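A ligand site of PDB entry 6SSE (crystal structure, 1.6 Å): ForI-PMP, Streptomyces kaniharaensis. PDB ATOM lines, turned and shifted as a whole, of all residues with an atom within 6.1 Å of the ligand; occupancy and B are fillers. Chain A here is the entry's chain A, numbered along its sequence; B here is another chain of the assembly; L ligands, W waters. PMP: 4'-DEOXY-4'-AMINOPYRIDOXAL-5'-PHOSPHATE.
Water W1 lies within hydrogen-bond range of O3 of the ligand (2.6 Å), O of Tyr 142 (3.0 Å) and NE1 of Trp 207 (3.2 Å).
Water W5 lies within hydrogen-bond range of O1P of the ligand, O of Ile 271, OH of Tyr 299 of chain B and N of Lys 263.
Water W6 bridges OE2 of Glu 117 of chain B (2.7 Å) and O2P of the ligand (2.8 Å).
Water W4 bridges an oxygen (O3P) of the ligand (2.8 Å) and the backbone NH (N) of Gly 297 of chain B (3.2 Å).
Ser 114 touches the ligand (CB to O2P, 3.5 Å).
Val 119 touches the ligand.
Tyr 142 touches the ligand.
His 143 touches the ligand.
Asp 203 touches the ligand.
Val 238 touches the ligand (CB to N1, 3.7 Å).
C of Gly 297 of chain B touches O3P of the ligand (3.7 Å).
CE2 of Tyr 299 of chain B touches O1P of the ligand, 3.6 Å away.
Hydrophobic or aromatic side chains within 4 Å of the ligand: Val 119, Tyr 142, Val 238 and Tyr 299 of chain B.
Within 4 Å of the ligand: Ser 114, Gly 115, Thr 116, Val 119, Tyr 142, His 143, Asp 203, Asp 236, Val 238, Lys 263, Gly 297 of chain B, Ser 298 of chain B and Tyr 299 of chain B.
The nearest printed residue that does not touch the ligand is Gly 144 (4.2 Å).
OG1 of Thr 116 lies within hydrogen-bond range of O2P of the ligand, 2.7 Å away.
O2P of the ligand sits at hydrogen-bond distance from N of Thr 116, 2.9 Å away.
The side-chain carboxylate of Asp 236 sits at hydrogen-bond distance from a nitrogen (N1) of the ligand (2.7 Å).
An oxygen (O1P) of the ligand sits at hydrogen-bond distance from the backbone NH (N) of Gly 115, at 2.8 Å.
N of Ser 298 of chain B lies within hydrogen-bond range of O3P of the ligand (2.8 Å).
NZ of Lys 263 lies close to O3 of the ligand (3.4 Å).
OG of Ser 298 of chain B lies within hydrogen-bond range of O3P of the ligand, at 2.6 Å.
N of Thr 116 lies close to OG of Ser 114 (3.4 Å).
ND1 of His 143 is in hydrogen-bond range of OD2 of Asp 236 (2.7 Å).
The side-chain carboxylate of Asp 203 lies within hydrogen-bond range of the side-chain hydroxyl of Ser 240.
The side-chain carboxylate (OD1) of Asp 236 sits at hydrogen-bond distance from the backbone NH (N) of Val 238 (3.0 Å).
OG of Ser 114 lies within hydrogen-bond range of OE2 of Glu 117 of chain B (2.6 Å).
N of Lys 263 is in hydrogen-bond range of OH of Tyr 299 of chain B (3.4 Å).
The side-chain hydroxyl (OG) of Ser 114 sits at hydrogen-bond distance from the backbone NH (N) of Glu 117 of chain A (3.0 Å).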
ATOM      1  N   SER A  59     -20.232  29.238  11.784  1.00  0.00           N
ATOM      2  CA  SER A  59     -18.791  29.496  12.016  1.00  0.00           C
ATOM      3  C   SER A  59     -18.357  30.766  11.249  1.00  0.00           C
ATOM      4  O   SER A  59     -17.297  30.801  10.623  1.00  0.00           O
ATOM      5  CB  SER A  59     -17.959  28.278  11.764  1.00  0.00           C
ATOM      6  OG  SER A  59     -17.817  28.003  10.385  1.00  0.00           O
ATOM      7  N   SER A 113     -14.073  25.050  -3.928  1.00  0.00           N
ATOM      8  CA  SER A 113     -15.365  24.761  -3.278  1.00  0.00           C
ATOM      9  C   SER A 113     -15.317  24.912  -1.759  1.00  0.00           C
ATOM     10  O   SER A 113     -16.370  24.672  -1.121  1.00  0.00           O
ATOM     11  CB  SER A 113     -15.824  23.421  -3.663  1.00  0.00           C
ATOM     12  OG  SER A 113     -16.230  23.445  -5.014  1.00  0.00           O
ATOM     13  N   SER A 114     -14.193  25.300  -1.197  1.00  0.00           N
ATOM     14  CA  SER A 114     -14.065  25.488   0.250  1.00  0.00           C
ATOM     15  C   SER A 114     -12.810  26.285   0.569  1.00  0.00           C
ATOM     16  O   SER A 114     -11.856  26.298  -0.212  1.00  0.00           O
ATOM     17  CB  SER A 114     -13.995  24.119   0.975  1.00  0.00           C
ATOM     18  OG  SER A 114     -12.775  23.456   0.664  1.00  0.00           O
ATOM     19  N   GLY A 115     -12.779  26.827   1.777  1.00  0.00           N
ATOM     20  CA  GLY A 115     -11.571  27.461   2.308  1.00  0.00           C
ATOM     21  C   GLY A 115     -10.477  26.446   2.497  1.00  0.00           C
ATOM     22  O   GLY A 115      -9.306  26.790   2.296  1.00  0.00           O
ATOM     23  N   THR A 116     -10.818  25.201   2.801  1.00  0.00           N
ATOM     24  CA  THR A 116      -9.808  24.164   3.016  1.00  0.00           C
ATOM     25  C   THR A 116      -9.068  23.912   1.712  1.00  0.00           C
ATOM     26  O   THR A 116      -7.840  23.850   1.727  1.00  0.00           O
ATOM     27  CB  THR A 116     -10.486  22.870   3.496  1.00  0.00           C
ATOM     28  OG1 THR A 116     -10.958  23.106   4.819  1.00  0.00           O
ATOM     29  CG2 THR A 116      -9.574  21.677   3.467  1.00  0.00           C
ATOM     30  N   GLU A 117      -9.761  23.831   0.609  1.00  0.00           N
ATOM     31  CA  GLU A 117      -9.142  23.646  -0.718  1.00  0.00           C
ATOM     32  C   GLU A 117      -8.373  24.925  -1.098  1.00  0.00           C
ATOM     33  O   GLU A 117      -7.315  24.843  -1.747  1.00  0.00           O
ATOM     34  CB  GLU A 117     -10.208  23.448  -1.800  1.00  0.00           C
ATOM     35  CG  GLU A 117     -10.873  22.074  -1.828  1.00  0.00           C
ATOM     36  CD  GLU A 117     -11.748  21.865  -3.069  1.00  0.00           C
ATOM     37  OE1 GLU A 117     -12.152  22.885  -3.760  1.00  0.00           O
ATOM     38  OE2 GLU A 117     -12.065  20.680  -3.339  1.00  0.00           O
ATOM     39  N   VAL A 119      -6.857  27.157   0.845  1.00  0.00           N
ATOM     40  CA  VAL A 119      -5.576  27.196   1.590  1.00  0.00           C
ATOM     41  C   VAL A 119      -4.619  26.219   0.908  1.00  0.00           C
ATOM     42  O   VAL A 119      -3.422  26.553   0.723  1.00  0.00           O
ATOM     43  CB  VAL A 119      -5.724  26.837   3.068  1.00  0.00           C
ATOM     44  CG1 VAL A 119      -4.345  26.699   3.737  1.00  0.00           C
ATOM     45  CG2 VAL A 119      -6.608  27.855   3.802  1.00  0.00           C
ATOM     46  N   TYR A 142      -5.450  27.653  13.161  1.00  0.00           N
ATOM     47  CA  TYR A 142      -6.175  26.611  12.394  1.00  0.00           C
ATOM     48  C   TYR A 142      -6.439  27.104  10.961  1.00  0.00           C
ATOM     49  O   TYR A 142      -6.851  28.275  10.751  1.00  0.00           O
ATOM     50  CB  TYR A 142      -7.520  26.302  13.041  1.00  0.00           C
ATOM     51  CG  TYR A 142      -8.254  25.168  12.369  1.00  0.00           C
ATOM     52  CD1 TYR A 142      -7.855  23.849  12.543  1.00  0.00           C
ATOM     53  CD2 TYR A 142      -9.338  25.402  11.549  1.00  0.00           C
ATOM     54  CE1 TYR A 142      -8.552  22.812  11.944  1.00  0.00           C
ATOM     55  CE2 TYR A 142     -10.059  24.370  10.967  1.00  0.00           C
ATOM     56  CZ  TYR A 142      -9.650  23.061  11.160  1.00  0.00           C
ATOM     57  OH  TYR A 142     -10.320  22.013  10.568  1.00  0.00           O
ATOM     58  N   HIS A 143      -6.162  26.226   9.985  1.00  0.00           N
ATOM     59  CA  HIS A 143      -6.352  26.499   8.536  1.00  0.00           C
ATOM     60  C   HIS A 143      -7.089  25.400   7.802  1.00  0.00           C
ATOM     61  O   HIS A 143      -6.929  25.349   6.577  1.00  0.00           O
ATOM     62  CB  HIS A 143      -5.011  26.755   7.901  1.00  0.00           C
ATOM     63  CG  HIS A 143      -4.245  27.892   8.494  1.00  0.00           C
ATOM     64  ND1 HIS A 143      -4.460  29.204   8.107  1.00  0.00           N
ATOM     65  CD2 HIS A 143      -3.287  27.905   9.452  1.00  0.00           C
ATOM     66  CE1 HIS A 143      -3.603  29.976   8.806  1.00  0.00           C
ATOM     67  NE2 HIS A 143      -2.824  29.197   9.600  1.00  0.00           N
ATOM     68  N   GLY A 144      -7.814  24.544   8.497  1.00  0.00           N
ATOM     69  CA  GLY A 144      -8.516  23.423   7.857  1.00  0.00           C
ATOM     70  C   GLY A 144      -7.679  22.140   7.872  1.00  0.00           C
ATOM     71  O   GLY A 144      -6.586  22.070   8.453  1.00  0.00           O
ATOM     72  N   ALA A 145      -8.216  21.100   7.254  1.00  0.00           N
ATOM     73  CA  ALA A 145      -7.710  19.719   7.385  1.00  0.00           C
ATOM     74  C   ALA A 145      -6.533  19.430   6.431  1.00  0.00           C
ATOM     75  O   ALA A 145      -5.933  18.343   6.624  1.00  0.00           O
ATOM     76  CB  ALA A 145      -8.857  18.739   7.159  1.00  0.00           C
ATOM     77  N   ASP A 203      -2.702  34.076   9.500  1.00  0.00           N
ATOM     78  CA  ASP A 203      -4.075  34.585   9.611  1.00  0.00           C
ATOM     79  C   ASP A 203      -3.888  35.863  10.391  1.00  0.00           C
ATOM     80  O   ASP A 203      -3.298  35.798  11.466  1.00  0.00           O
ATOM     81  CB  ASP A 203      -4.977  33.574  10.280  1.00  0.00           C
ATOM     82  CG  ASP A 203      -6.412  34.029  10.542  1.00  0.00           C
ATOM     83  OD1 ASP A 203      -6.726  35.257  10.404  1.00  0.00           O
ATOM     84  OD2 ASP A 203      -7.244  33.122  10.809  1.00  0.00           O
ATOM     85  N   TRP A 207      -8.591  33.073  15.262  1.00  0.00           N
ATOM     86  CA  TRP A 207      -9.508  32.918  16.407  1.00  0.00           C
ATOM     87  C   TRP A 207      -9.015  31.827  17.378  1.00  0.00           C
ATOM     88  O   TRP A 207      -9.279  31.983  18.583  1.00  0.00           O
ATOM     89  CB  TRP A 207     -10.940  32.681  15.952  1.00  0.00           C
ATOM     90  CG  TRP A 207     -11.265  31.279  15.592  1.00  0.00           C
ATOM     91  CD1 TRP A 207     -11.272  30.738  14.334  1.00  0.00           C
ATOM     92  CD2 TRP A 207     -11.709  30.230  16.478  1.00  0.00           C
ATOM     93  NE1 TRP A 207     -11.633  29.410  14.387  1.00  0.00           N
ATOM     94  CE2 TRP A 207     -11.927  29.079  15.692  1.00  0.00           C
ATOM     95  CE3 TRP A 207     -11.900  30.145  17.858  1.00  0.00           C
ATOM     96  CZ2 TRP A 207     -12.348  27.861  16.228  1.00  0.00           C
ATOM     97  CZ3 TRP A 207     -12.362  28.956  18.382  1.00  0.00           C
ATOM     98  CH2 TRP A 207     -12.548  27.822  17.586  1.00  0.00           C
ATOM     99  N   ASP A 236      -4.308  34.050   5.167  1.00  0.00           N
ATOM    100  CA  ASP A 236      -5.545  33.225   5.223  1.00  0.00           C
ATOM    101  C   ASP A 236      -6.621  34.029   5.934  1.00  0.00           C
ATOM    102  O   ASP A 236      -6.587  34.146   7.178  1.00  0.00           O
ATOM    103  CB  ASP A 236      -5.276  31.877   5.865  1.00  0.00           C
ATOM    104  CG  ASP A 236      -6.570  31.056   5.974  1.00  0.00           C
ATOM    105  OD1 ASP A 236      -7.622  31.535   5.512  1.00  0.00           O
ATOM    106  OD2 ASP A 236      -6.508  29.900   6.487  1.00  0.00           O
ATOM    107  N   GLU A 237      -7.493  34.627   5.142  1.00  0.00           N
ATOM    108  CA  GLU A 237      -8.614  35.457   5.632  1.00  0.00           C
ATOM    109  C   GLU A 237      -9.930  34.731   5.412  1.00  0.00           C
ATOM    110  O   GLU A 237     -10.990  35.380   5.467  1.00  0.00           O
ATOM    111  CB  GLU A 237      -8.575  36.811   4.936  1.00  0.00           C
ATOM    112  CG  GLU A 237      -7.290  37.529   5.216  1.00  0.00           C
ATOM    113  CD  GLU A 237      -7.214  38.959   4.777  1.00  0.00           C
ATOM    114  OE1 GLU A 237      -8.270  39.537   4.465  1.00  0.00           O
ATOM    115  OE2 GLU A 237      -6.060  39.456   4.742  1.00  0.00           O
ATOM    116  N   VAL A 238      -9.960  33.414   5.371  1.00  0.00           N
ATOM    117  CA  VAL A 238     -11.230  32.676   5.264  1.00  0.00           C
ATOM    118  C   VAL A 238     -12.171  33.105   6.381  1.00  0.00           C
ATOM    119  O   VAL A 238     -13.355  33.329   6.081  1.00  0.00           O
ATOM    120  CB  VAL A 238     -10.991  31.158   5.228  1.00  0.00           C
ATOM    121  CG1 VAL A 238     -12.332  30.446   5.313  1.00  0.00           C
ATOM    122  CG2 VAL A 238     -10.290  30.724   3.934  1.00  0.00           C
ATOM    123  N   GLY A 239     -11.697  33.217   7.613  1.00  0.00           N
ATOM    124  CA  GLY A 239     -12.535  33.739   8.710  1.00  0.00           C
ATOM    125  C   GLY A 239     -12.372  35.245   8.959  1.00  0.00           C
ATOM    126  O   GLY A 239     -13.322  35.878   9.398  1.00  0.00           O
ATOM    127  N   SER A 240     -11.172  35.769   8.830  1.00  0.00           N
ATOM    128  CA  SER A 240     -10.875  37.125   9.355  1.00  0.00           C
ATOM    129  C   SER A 240     -11.148  38.179   8.289  1.00  0.00           C
ATOM    130  O   SER A 240     -11.162  39.356   8.610  1.00  0.00           O
ATOM    131  CB  SER A 240      -9.433  37.205   9.842  1.00  0.00           C
ATOM    132  OG  SER A 240      -8.519  36.755   8.841  1.00  0.00           O
ATOM    133  N   GLY A 262     -12.982  32.885   1.851  1.00  0.00           N
ATOM    134  CA  GLY A 262     -14.130  31.988   1.823  1.00  0.00           C
ATOM    135  C   GLY A 262     -15.233  32.562   2.682  1.00  0.00           C
ATOM    136  O   GLY A 262     -15.348  33.794   2.788  1.00  0.00           O
ATOM    137  N   LYS A 263     -16.073  31.686   3.210  1.00  0.00           N
ATOM    138  CA  LYS A 263     -17.113  32.051   4.205  1.00  0.00           C
ATOM    139  C   LYS A 263     -17.914  33.266   3.744  1.00  0.00           C
ATOM    140  O   LYS A 263     -18.766  33.061   2.828  1.00  0.00           O
ATOM    141  CB  LYS A 263     -16.441  32.203   5.569  1.00  0.00           C
ATOM    142  CG  LYS A 263     -16.063  30.851   6.174  1.00  0.00           C
ATOM    143  CD  LYS A 263     -15.709  30.954   7.643  1.00  0.00           C
ATOM    144  CE  LYS A 263     -15.405  29.615   8.298  1.00  0.00           C
ATOM    145  NZ  LYS A 263     -13.969  29.488   8.576  1.00  0.00           N
ATOM    146  N   ILE A 271     -17.762  27.680  -1.133  1.00  0.00           N
ATOM    147  CA  ILE A 271     -16.822  28.627  -1.801  1.00  0.00           C
ATOM    148  C   ILE A 271     -15.474  28.612  -1.105  1.00  0.00           C
ATOM    149  O   ILE A 271     -15.405  28.489   0.154  1.00  0.00           O
ATOM    150  CB  ILE A 271     -17.410  30.073  -1.803  1.00  0.00           C
ATOM    151  CG1 ILE A 271     -16.703  30.995  -2.798  1.00  0.00           C
ATOM    152  CG2 ILE A 271     -17.378  30.674  -0.402  1.00  0.00           C
ATOM    153  CD1 ILE A 271     -16.673  30.471  -4.221  1.00  0.00           C
ATOM    154  N   GLU B 117     -11.585  16.728  -1.552  1.00  0.00           N
ATOM    155  CA  GLU B 117     -11.531  16.686  -0.087  1.00  0.00           C
ATOM    156  C   GLU B 117     -11.804  15.251   0.411  1.00  0.00           C
ATOM    157  O   GLU B 117     -11.225  14.851   1.424  1.00  0.00           O
ATOM    158  CB  GLU B 117     -12.606  17.598   0.544  1.00  0.00           C
ATOM    159  CG  GLU B 117     -12.286  19.077   0.520  1.00  0.00           C
ATOM    160  CD  GLU B 117     -13.284  19.901   1.361  1.00  0.00           C
ATOM    161  OE1 GLU B 117     -14.458  19.404   1.705  1.00  0.00           O
ATOM    162  OE2 GLU B 117     -12.981  21.083   1.640  1.00  0.00           O
ATOM    163  N   SER B 296     -13.575  18.802   9.964  1.00  0.00           N
ATOM    164  CA  SER B 296     -14.589  19.851   9.923  1.00  0.00           C
ATOM    165  C   SER B 296     -14.713  20.332   8.492  1.00  0.00           C
ATOM    166  O   SER B 296     -14.259  19.607   7.531  1.00  0.00           O
ATOM    167  CB  SER B 296     -14.318  20.850  10.942  1.00  0.00           C
ATOM    168  OG  SER B 296     -14.454  20.271  12.249  1.00  0.00           O
ATOM    169  N   GLY B 297     -15.299  21.502   8.300  1.00  0.00           N
ATOM    170  CA  GLY B 297     -15.546  22.063   6.967  1.00  0.00           C
ATOM    171  C   GLY B 297     -16.866  22.787   6.979  1.00  0.00           C
ATOM    172  O   GLY B 297     -17.889  22.168   7.312  1.00  0.00           O
ATOM    173  N   SER B 298     -16.863  24.061   6.600  1.00  0.00           N
ATOM    174  CA  SER B 298     -18.036  24.943   6.758  1.00  0.00           C
ATOM    175  C   SER B 298     -19.237  24.373   6.044  1.00  0.00           C
ATOM    176  O   SER B 298     -20.368  24.704   6.442  1.00  0.00           O
ATOM    177  CB  SER B 298     -17.698  26.345   6.256  1.00  0.00           C
ATOM    178  OG  SER B 298     -16.658  26.848   7.090  1.00  0.00           O
ATOM    179  N   TYR B 299     -19.066  23.701   4.918  1.00  0.00           N
ATOM    180  CA  TYR B 299     -20.199  23.245   4.091  1.00  0.00           C
ATOM    181  C   TYR B 299     -20.442  21.733   4.196  1.00  0.00           C
ATOM    182  O   TYR B 299     -21.323  21.212   3.503  1.00  0.00           O
ATOM    183  CB  TYR B 299     -20.056  23.717   2.656  1.00  0.00           C
ATOM    184  CG  TYR B 299     -19.547  25.137   2.579  1.00  0.00           C
ATOM    185  CD1 TYR B 299     -20.392  26.205   2.837  1.00  0.00           C
ATOM    186  CD2 TYR B 299     -18.216  25.393   2.391  1.00  0.00           C
ATOM    187  CE1 TYR B 299     -19.933  27.502   2.879  1.00  0.00           C
ATOM    188  CE2 TYR B 299     -17.729  26.695   2.414  1.00  0.00           C
ATOM    189  CZ  TYR B 299     -18.589  27.741   2.696  1.00  0.00           C
ATOM    190  OH  TYR B 299     -18.106  29.018   2.694  1.00  0.00           O
HETATM  191  N1  PMP L   1      -8.858  28.834   7.142  1.00  0.00           N
HETATM  192  C2  PMP L   1      -9.336  29.313   8.297  1.00  0.00           C
HETATM  193  C2A PMP L   1      -8.565  30.407   8.974  1.00  0.00           C
HETATM  194  C3  PMP L   1     -10.495  28.794   8.857  1.00  0.00           C
HETATM  195  O3  PMP L   1     -10.931  29.209  10.087  1.00  0.00           O
HETATM  196  C4  PMP L   1     -11.187  27.769   8.215  1.00  0.00           C
HETATM  197  C4A PMP L   1     -12.413  27.120   8.810  1.00  0.00           C
HETATM  198  N4A PMP L   1     -12.443  27.264  10.268  1.00  0.00           N
HETATM  199  C5  PMP L   1     -10.668  27.265   7.030  1.00  0.00           C
HETATM  200  C6  PMP L   1      -9.529  27.856   6.500  1.00  0.00           C
HETATM  201  C5A PMP L   1     -11.398  26.188   6.312  1.00  0.00           C
HETATM  202  O4P PMP L   1     -12.414  26.756   5.457  1.00  0.00           O
HETATM  203  P   PMP L   1     -13.738  25.854   5.000  1.00  0.00           P
HETATM  204  O1P PMP L   1     -14.450  26.723   3.963  1.00  0.00           O
HETATM  205  O2P PMP L   1     -13.189  24.608   4.342  1.00  0.00           O
HETATM  206  O3P PMP L   1     -14.517  25.596   6.262  1.00  0.00           O
HETATM  207  O   HOH W   1      -9.320  29.204  12.180  1.00  0.00           O
HETATM  208  O   HOH W   2      -8.998  33.698   8.603  1.00  0.00           O
HETATM  209  O   HOH W   3     -11.491  31.524  11.042  1.00  0.00           O
HETATM  210  O   HOH W   4     -13.896  24.367   8.681  1.00  0.00           O
HETATM  211  O   HOH W   5     -15.363  28.962   2.818  1.00  0.00           O
HETATM  212  O   HOH W   6     -14.346  22.149   3.755  1.00  0.00           O
